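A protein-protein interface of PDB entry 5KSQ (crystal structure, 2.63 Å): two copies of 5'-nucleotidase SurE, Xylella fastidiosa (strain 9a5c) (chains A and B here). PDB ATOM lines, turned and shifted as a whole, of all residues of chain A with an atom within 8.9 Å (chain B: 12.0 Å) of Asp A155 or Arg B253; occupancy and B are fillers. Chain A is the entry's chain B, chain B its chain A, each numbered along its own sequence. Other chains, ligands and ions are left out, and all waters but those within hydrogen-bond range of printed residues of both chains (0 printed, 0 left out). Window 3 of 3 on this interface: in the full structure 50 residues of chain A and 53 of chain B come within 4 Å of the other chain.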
ATOM      1  N   ASN A 147      10.705  -2.073  -3.678  1.00  0.00           N
ATOM      2  CA  ASN A 147       9.384  -2.651  -3.456  1.00  0.00           C
ATOM      3  C   ASN A 147       9.075  -3.791  -4.423  1.00  0.00           C
ATOM      4  O   ASN A 147       8.466  -4.790  -4.043  1.00  0.00           O
ATOM      5  CB  ASN A 147       8.301  -1.573  -3.540  1.00  0.00           C
ATOM      6  CG  ASN A 147       8.344  -0.611  -2.368  1.00  0.00           C
ATOM      7  OD1 ASN A 147       7.697  -0.834  -1.345  1.00  0.00           O
ATOM      8  ND2 ASN A 147       9.108   0.464  -2.511  1.00  0.00           N
ATOM      9  N   ILE A 148       9.499  -3.633  -5.672  1.00  0.00           N
ATOM     10  CA  ILE A 148       9.292  -4.660  -6.687  1.00  0.00           C
ATOM     11  C   ILE A 148      10.106  -5.909  -6.363  1.00  0.00           C
ATOM     12  O   ILE A 148       9.625  -7.034  -6.522  1.00  0.00           O
ATOM     13  CB  ILE A 148       9.669  -4.142  -8.089  1.00  0.00           C
ATOM     14  CG1 ILE A 148       8.827  -2.915  -8.444  1.00  0.00           C
ATOM     15  CG2 ILE A 148       9.486  -5.232  -9.135  1.00  0.00           C
ATOM     16  CD1 ILE A 148       9.173  -2.300  -9.780  1.00  0.00           C
ATOM     17  N   VAL A 149      11.335  -5.702  -5.899  1.00  0.00           N
ATOM     18  CA  VAL A 149      12.223  -6.800  -5.528  1.00  0.00           C
ATOM     19  C   VAL A 149      11.650  -7.634  -4.382  1.00  0.00           C
ATOM     20  O   VAL A 149      11.656  -8.866  -4.433  1.00  0.00           O
ATOM     21  CB  VAL A 149      13.621  -6.276  -5.135  1.00  0.00           C
ATOM     22  CG1 VAL A 149      14.454  -7.382  -4.506  1.00  0.00           C
ATOM     23  CG2 VAL A 149      14.328  -5.691  -6.347  1.00  0.00           C
ATOM     24  N   ALA A 150      11.145  -6.955  -3.357  1.00  0.00           N
ATOM     25  CA  ALA A 150      10.588  -7.630  -2.191  1.00  0.00           C
ATOM     26  C   ALA A 150       9.308  -8.391  -2.530  1.00  0.00           C
ATOM     27  O   ALA A 150       8.934  -9.334  -1.832  1.00  0.00           O
ATOM     28  CB  ALA A 150      10.333  -6.633  -1.070  1.00  0.00           C
ATOM     29  N   GLN A 151       8.642  -7.978  -3.604  1.00  0.00           N
ATOM     30  CA  GLN A 151       7.410  -8.630  -4.035  1.00  0.00           C
ATOM     31  C   GLN A 151       7.713  -9.857  -4.890  1.00  0.00           C
ATOM     32  O   GLN A 151       6.971 -10.839  -4.868  1.00  0.00           O
ATOM     33  CB  GLN A 151       6.527  -7.647  -4.808  1.00  0.00           C
ATOM     34  CG  GLN A 151       5.126  -8.164  -5.104  1.00  0.00           C
ATOM     35  CD  GLN A 151       4.251  -8.235  -3.867  1.00  0.00           C
ATOM     36  OE1 GLN A 151       4.572  -7.654  -2.830  1.00  0.00           O
ATOM     37  NE2 GLN A 151       3.137  -8.950  -3.971  1.00  0.00           N
ATOM     38  N   LEU A 152       8.808  -9.794  -5.643  1.00  0.00           N
ATOM     39  CA  LEU A 152       9.239 -10.915  -6.472  1.00  0.00           C
ATOM     40  C   LEU A 152       9.754 -12.068  -5.618  1.00  0.00           C
ATOM     41  O   LEU A 152       9.742 -13.223  -6.045  1.00  0.00           O
ATOM     42  CB  LEU A 152      10.323 -10.473  -7.458  1.00  0.00           C
ATOM     43  CG  LEU A 152       9.880  -9.604  -8.635  1.00  0.00           C
ATOM     44  CD1 LEU A 152      11.082  -9.161  -9.455  1.00  0.00           C
ATOM     45  CD2 LEU A 152       8.888 -10.355  -9.505  1.00  0.00           C
ATOM     46  N   LYS A 153      10.210 -11.744  -4.411  1.00  0.00           N
ATOM     47  CA  LYS A 153      10.736 -12.746  -3.492  1.00  0.00           C
ATOM     48  C   LYS A 153       9.634 -13.680  -3.005  1.00  0.00           C
ATOM     49  O   LYS A 153       9.781 -14.902  -3.044  1.00  0.00           O
ATOM     50  CB  LYS A 153      11.416 -12.070  -2.300  1.00  0.00           C
ATOM     51  N   THR A 154       8.532 -13.098  -2.547  1.00  0.00           N
ATOM     52  CA  THR A 154       7.409 -13.876  -2.035  1.00  0.00           C
ATOM     53  C   THR A 154       6.518 -14.382  -3.166  1.00  0.00           C
ATOM     54  O   THR A 154       6.069 -15.528  -3.148  1.00  0.00           O
ATOM     55  CB  THR A 154       6.556 -13.053  -1.053  1.00  0.00           C
ATOM     56  OG1 THR A 154       5.979 -11.934  -1.738  1.00  0.00           O
ATOM     57  CG2 THR A 154       7.408 -12.550   0.102  1.00  0.00           C
ATOM     58  N   ASP A 155       6.267 -13.521  -4.146  1.00  0.00           N
ATOM     59  CA  ASP A 155       5.422 -13.876  -5.280  1.00  0.00           C
ATOM     60  C   ASP A 155       6.218 -13.799  -6.580  1.00  0.00           C
ATOM     61  O   ASP A 155       6.255 -12.754  -7.228  1.00  0.00           O
ATOM     62  CB  ASP A 155       4.207 -12.946  -5.347  1.00  0.00           C
ATOM     63  CG  ASP A 155       3.072 -13.521  -6.177  1.00  0.00           C
ATOM     64  OD1 ASP A 155       3.342 -14.322  -7.097  1.00  0.00           O
ATOM     65  OD2 ASP A 155       1.905 -13.167  -5.908  1.00  0.00           O
ATOM     66  N   PRO A 156       6.859 -14.914  -6.964  1.00  0.00           N
ATOM     67  CA  PRO A 156       7.689 -14.968  -8.173  1.00  0.00           C
ATOM     68  C   PRO A 156       6.864 -14.953  -9.457  1.00  0.00           C
ATOM     69  O   PRO A 156       5.650 -15.157  -9.422  1.00  0.00           O
ATOM     70  CB  PRO A 156       8.415 -16.306  -8.031  1.00  0.00           C
ATOM     71  CG  PRO A 156       7.492 -17.143  -7.220  1.00  0.00           C
ATOM     72  CD  PRO A 156       6.845 -16.200  -6.247  1.00  0.00           C
ATOM     73  N   LEU A 157       7.531 -14.713 -10.581  1.00  0.00           N
ATOM     74  CA  LEU A 157       6.880 -14.678 -11.885  1.00  0.00           C
ATOM     75  C   LEU A 157       7.281 -15.908 -12.703  1.00  0.00           C
ATOM     76  O   LEU A 157       8.230 -16.605 -12.338  1.00  0.00           O
ATOM     77  CB  LEU A 157       7.261 -13.385 -12.617  1.00  0.00           C
ATOM     78  N   PRO A 158       6.553 -16.192 -13.804  1.00  0.00           N
ATOM     79  CA  PRO A 158       6.901 -17.280 -14.729  1.00  0.00           C
ATOM     80  C   PRO A 158       8.359 -17.265 -15.192  1.00  0.00           C
ATOM     81  O   PRO A 158       8.849 -18.281 -15.688  1.00  0.00           O
ATOM     82  CB  PRO A 158       5.972 -17.025 -15.915  1.00  0.00           C
ATOM     83  CG  PRO A 158       4.757 -16.449 -15.290  1.00  0.00           C
ATOM     84  CD  PRO A 158       5.236 -15.611 -14.130  1.00  0.00           C
ATOM     85  N   LEU A 163      11.179  -7.306 -16.921  1.00  0.00           N
ATOM     86  CA  LEU A 163      10.343  -6.128 -16.718  1.00  0.00           C
ATOM     87  C   LEU A 163      11.078  -4.830 -17.046  1.00  0.00           C
ATOM     88  O   LEU A 163      12.213  -4.621 -16.617  1.00  0.00           O
ATOM     89  CB  LEU A 163       9.826  -6.081 -15.279  1.00  0.00           C
ATOM     90  CG  LEU A 163       8.994  -7.275 -14.807  1.00  0.00           C
ATOM     91  CD1 LEU A 163       8.553  -7.083 -13.365  1.00  0.00           C
ATOM     92  CD2 LEU A 163       7.793  -7.489 -15.716  1.00  0.00           C
ATOM     93  N   ALA B 243       1.266 -12.327 -21.385  1.00  0.00           N
ATOM     94  CA  ALA B 243       1.668 -12.231 -19.986  1.00  0.00           C
ATOM     95  C   ALA B 243       1.014 -11.036 -19.297  1.00  0.00           C
ATOM     96  O   ALA B 243       1.232 -10.799 -18.110  1.00  0.00           O
ATOM     97  CB  ALA B 243       3.182 -12.144 -19.874  1.00  0.00           C
ATOM     98  N   LEU B 244       0.207 -10.292 -20.047  1.00  0.00           N
ATOM     99  CA  LEU B 244      -0.427  -9.083 -19.530  1.00  0.00           C
ATOM    100  C   LEU B 244      -1.469  -9.372 -18.450  1.00  0.00           C
ATOM    101  O   LEU B 244      -1.811  -8.492 -17.659  1.00  0.00           O
ATOM    102  CB  LEU B 244      -1.063  -8.282 -20.670  1.00  0.00           C
ATOM    103  CG  LEU B 244      -0.114  -7.721 -21.731  1.00  0.00           C
ATOM    104  CD1 LEU B 244      -0.892  -7.011 -22.829  1.00  0.00           C
ATOM    105  CD2 LEU B 244       0.905  -6.781 -21.102  1.00  0.00           C
ATOM    106  N   GLU B 245      -1.968 -10.604 -18.417  1.00  0.00           N
ATOM    107  CA  GLU B 245      -2.999 -10.983 -17.456  1.00  0.00           C
ATOM    108  C   GLU B 245      -2.435 -11.224 -16.057  1.00  0.00           C
ATOM    109  O   GLU B 245      -3.012 -10.783 -15.063  1.00  0.00           O
ATOM    110  CB  GLU B 245      -3.758 -12.221 -17.939  1.00  0.00           C
ATOM    111  N   ASN B 246      -1.308 -11.925 -15.984  1.00  0.00           N
ATOM    112  CA  ASN B 246      -0.696 -12.256 -14.701  1.00  0.00           C
ATOM    113  C   ASN B 246      -0.025 -11.065 -14.024  1.00  0.00           C
ATOM    114  O   ASN B 246      -0.100 -10.913 -12.805  1.00  0.00           O
ATOM    115  CB  ASN B 246       0.304 -13.404 -14.860  1.00  0.00           C
ATOM    116  CG  ASN B 246      -0.372 -14.725 -15.174  1.00  0.00           C
ATOM    117  OD1 ASN B 246      -1.527 -14.759 -15.599  1.00  0.00           O
ATOM    118  ND2 ASN B 246       0.347 -15.821 -14.963  1.00  0.00           N
ATOM    119  N   VAL B 247       0.629 -10.224 -14.818  1.00  0.00           N
ATOM    120  CA  VAL B 247       1.327  -9.054 -14.292  1.00  0.00           C
ATOM    121  C   VAL B 247       0.340  -8.034 -13.720  1.00  0.00           C
ATOM    122  O   VAL B 247       0.636  -7.356 -12.735  1.00  0.00           O
ATOM    123  CB  VAL B 247       2.208  -8.393 -15.377  1.00  0.00           C
ATOM    124  CG1 VAL B 247       2.954  -7.194 -14.812  1.00  0.00           C
ATOM    125  CG2 VAL B 247       3.189  -9.405 -15.947  1.00  0.00           C
ATOM    126  N   THR B 248      -0.835  -7.943 -14.333  1.00  0.00           N
ATOM    127  CA  THR B 248      -1.875  -7.029 -13.873  1.00  0.00           C
ATOM    128  C   THR B 248      -2.340  -7.378 -12.461  1.00  0.00           C
ATOM    129  O   THR B 248      -2.423  -6.509 -11.593  1.00  0.00           O
ATOM    130  CB  THR B 248      -3.090  -7.033 -14.820  1.00  0.00           C
ATOM    131  OG1 THR B 248      -2.681  -6.621 -16.130  1.00  0.00           O
ATOM    132  CG2 THR B 248      -4.168  -6.088 -14.310  1.00  0.00           C
ATOM    133  N   ARG B 249      -2.641  -8.655 -12.239  1.00  0.00           N
ATOM    134  CA  ARG B 249      -3.071  -9.124 -10.927  1.00  0.00           C
ATOM    135  C   ARG B 249      -1.924  -9.043  -9.923  1.00  0.00           C
ATOM    136  O   ARG B 249      -2.140  -8.813  -8.732  1.00  0.00           O
ATOM    137  CB  ARG B 249      -3.590 -10.560 -11.013  1.00  0.00           C
ATOM    138  CG  ARG B 249      -4.739 -10.750 -11.990  1.00  0.00           C
ATOM    139  CD  ARG B 249      -5.144 -12.213 -12.084  1.00  0.00           C
ATOM    140  N   TRP B 250      -0.705  -9.233 -10.418  1.00  0.00           N
ATOM    141  CA  TRP B 250       0.487  -9.164  -9.584  1.00  0.00           C
ATOM    142  C   TRP B 250       0.735  -7.737  -9.107  1.00  0.00           C
ATOM    143  O   TRP B 250       1.190  -7.517  -7.985  1.00  0.00           O
ATOM    144  CB  TRP B 250       1.701  -9.682 -10.361  1.00  0.00           C
ATOM    145  CG  TRP B 250       2.987  -9.650  -9.591  1.00  0.00           C
ATOM    146  CD1 TRP B 250       3.483 -10.630  -8.783  1.00  0.00           C
ATOM    147  CD2 TRP B 250       3.946  -8.587  -9.569  1.00  0.00           C
ATOM    148  NE1 TRP B 250       4.690 -10.242  -8.254  1.00  0.00           N
ATOM    149  CE2 TRP B 250       4.997  -8.992  -8.721  1.00  0.00           C
ATOM    150  CE3 TRP B 250       4.018  -7.331 -10.180  1.00  0.00           C
ATOM    151  CZ2 TRP B 250       6.106  -8.185  -8.470  1.00  0.00           C
ATOM    152  CZ3 TRP B 250       5.119  -6.533  -9.929  1.00  0.00           C
ATOM    153  CH2 TRP B 250       6.148  -6.963  -9.081  1.00  0.00           C
ATOM    154  N   THR B 251       0.427  -6.770  -9.966  1.00  0.00           N
ATOM    155  CA  THR B 251       0.632  -5.361  -9.651  1.00  0.00           C
ATOM    156  C   THR B 251      -0.419  -4.859  -8.661  1.00  0.00           C
ATOM    157  O   THR B 251      -0.161  -3.950  -7.871  1.00  0.00           O
ATOM    158  CB  THR B 251       0.604  -4.492 -10.928  1.00  0.00           C
ATOM    159  OG1 THR B 251       1.459  -5.069 -11.923  1.00  0.00           O
ATOM    160  CG2 THR B 251       1.069  -3.075 -10.630  1.00  0.00           C
ATOM    161  N   ASP B 252      -1.603  -5.464  -8.701  1.00  0.00           N
ATOM    162  CA  ASP B 252      -2.683  -5.087  -7.793  1.00  0.00           C
ATOM    163  C   ASP B 252      -2.348  -5.427  -6.344  1.00  0.00           C
ATOM    164  O   ASP B 252      -2.664  -4.662  -5.432  1.00  0.00           O
ATOM    165  CB  ASP B 252      -3.997  -5.758  -8.204  1.00  0.00           C
ATOM    166  CG  ASP B 252      -4.550  -5.208  -9.505  1.00  0.00           C
ATOM    167  OD1 ASP B 252      -4.263  -4.037  -9.826  1.00  0.00           O
ATOM    168  OD2 ASP B 252      -5.275  -5.947 -10.203  1.00  0.00           O
ATOM    169  N   ARG B 253      -1.708  -6.573  -6.136  1.00  0.00           N
ATOM    170  CA  ARG B 253      -1.299  -6.983  -4.797  1.00  0.00           C
ATOM    171  C   ARG B 253      -0.122  -6.144  -4.309  1.00  0.00           C
ATOM    172  O   ARG B 253       0.071  -5.967  -3.106  1.00  0.00           O
ATOM    173  CB  ARG B 253      -0.941  -8.471  -4.766  1.00  0.00           C
ATOM    174  CG  ARG B 253      -2.111  -9.397  -5.057  1.00  0.00           C
ATOM    175  CD  ARG B 253      -1.734 -10.853  -4.836  1.00  0.00           C
ATOM    176  NE  ARG B 253      -0.623 -11.270  -5.688  1.00  0.00           N
ATOM    177  CZ  ARG B 253      -0.769 -11.801  -6.898  1.00  0.00           C
ATOM    178  NH1 ARG B 253      -1.981 -11.981  -7.405  1.00  0.00           N
ATOM    179  NH2 ARG B 253       0.299 -12.152  -7.602  1.00  0.00           N
ATOM    180  N   LEU B 254       0.663  -5.630  -5.252  1.00  0.00           N
ATOM    181  CA  LEU B 254       1.774  -4.744  -4.928  1.00  0.00           C
ATOM    182  C   LEU B 254       1.250  -3.413  -4.401  1.00  0.00           C
ATOM    183  O   LEU B 254       1.775  -2.867  -3.432  1.00  0.00           O
ATOM    184  CB  LEU B 254       2.653  -4.513  -6.159  1.00  0.00           C
ATOM    185  CG  LEU B 254       3.780  -3.490  -6.012  1.00  0.00           C
ATOM    186  CD1 LEU B 254       4.735  -3.893  -4.898  1.00  0.00           C
ATOM    187  CD2 LEU B 254       4.526  -3.319  -7.327  1.00  0.00           C
ATOM    188  N   THR B 255       0.209  -2.901  -5.050  1.00  0.00           N
ATOM    189  CA  THR B 255      -0.420  -1.656  -4.631  1.00  0.00           C
ATOM    190  C   THR B 255      -1.127  -1.851  -3.294  1.00  0.00           C
ATOM    191  O   THR B 255      -1.166  -0.945  -2.460  1.00  0.00           O
ATOM    192  CB  THR B 255      -1.436  -1.162  -5.681  1.00  0.00           C
ATOM    193  OG1 THR B 255      -0.800  -1.082  -6.963  1.00  0.00           O
ATOM    194  CG2 THR B 255      -1.980   0.207  -5.303  1.00  0.00           C
ATOM    195  N   ALA B 256      -1.672  -3.046  -3.091  1.00  0.00           N
ATOM    196  CA  ALA B 256      -2.375  -3.370  -1.855  1.00  0.00           C
ATOM    197  C   ALA B 256      -1.421  -3.903  -0.790  1.00  0.00           C
ATOM    198  O   ALA B 256      -1.648  -4.970  -0.218  1.00  0.00           O
ATOM    199  CB  ALA B 256      -3.486  -4.374  -2.126  1.00  0.00           C
ATOM    200  N   HIS B 257      -0.355  -3.154  -0.528  1.00  0.00           N
ATOM    201  CA  HIS B 257       0.612  -3.527   0.499  1.00  0.00           C
ATOM    202  C   HIS B 257       0.924  -2.324   1.384  1.00  0.00           C
ATOM    203  O   HIS B 257       2.085  -1.965   1.582  1.00  0.00           O
ATOM    204  CB  HIS B 257       1.893  -4.069  -0.141  1.00  0.00           C
ATOM    205  N   MET B 258      -0.127  -1.701   1.910  1.00  0.00           N
ATOM    206  CA  MET B 258       0.020  -0.523   2.757  1.00  0.00           C
ATOM    207  C   MET B 258      -0.730  -0.697   4.073  1.00  0.00           C
ATOM    208  O   MET B 258      -0.123  -0.898   5.124  1.00  0.00           O
ATOM    209  CB  MET B 258      -0.481   0.726   2.028  1.00  0.00           C
ATOM    210  CG  MET B 258       0.248   1.022   0.725  1.00  0.00           C
ATOM    211  SD  MET B 258      -0.391   2.479  -0.123  1.00  0.00           S
ATOM    212  CE  MET B 258      -0.072   3.752   1.096  1.00  0.00           C
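The backbone carbonyl oxygen (O) of Asp A155 is in hydrogen-bond range of the indole nitrogen (NE1) of Trp B250, 3.1 Å away.
NH2 of Arg B253 lies within salt-bridge range of OD2 of Asp A155, 2.5 Å away.
Printed residues of chain A that touch a printed residue of chain B: Asn A147, Ile A148, Gln A151, Leu A152 and Asp A155.
Of the 16 printed residues of chain B, 3 touch a printed residue of chain A.
Hydrophobic or aromatic side chains of chain B within 4 Å of the printed part of chain A: Trp B250 and Leu B254.
Among the printed residues, Asp or Glu carboxylates within 4 Å of a Lys or Arg side-chain nitrogen of the other chain: Asp A155 with Arg B253.
Among the printed residues, merely in contact across the chains: Asn A147 with Leu B254 (3.9 Å), Ile A148 with Trp B250 (3.8 Å), Gln A151 with Trp B250 (3.5 Å) and Leu A152 with Trp B250 (3.7 Å).
O of Arg B249 is in hydrogen-bond range of NH1 of Arg B253, at 3.4 Å.
The side-chain hydroxyl of Thr A154 lies within hydrogen-bond range of the backbone carbonyl oxygen of Gln A151, at 3.5 Å.
Printed residues of chain B within 4 Å of Asn A147: Leu B254.
Of the printed residues of chain B, Ile A148 touches Trp B250 (3.8 Å).
Ala A150 touches none of the printed residues of chain B.
Gln A151 touches just one residue of chain B: Trp B250.
Of chain B, only Trp B250 comes within 4 Å of Leu A152.
No residue of chain B comes within 4 Å of Thr A154.
Of chain B, only Trp B250 (3.1 Å) and Arg B253 (2.5 Å) come within 4 Å of Asp A155.
No residue of chain B comes within 4 Å of Pro A156.
No residue of chain B comes within 4 Å of Leu A157.
Glu B245 touches none of the printed residues of chain A.
Of the printed residues of chain A, Trp B250 touches Ile A148 (3.8 Å), Gln A151 (3.5 Å), Leu A152 (3.7 Å) and Asp A155 (3.1 Å).
Printed residues of chain A within 4 Å of Leu B254: Asn A147 (3.9 Å).
No residue of chain A comes within 4 Å of Ala B256.
The nearest printed residue of chain A that does not touch Trp B250 is Leu A163 (4.9 Å).
No position is printed for both chains.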
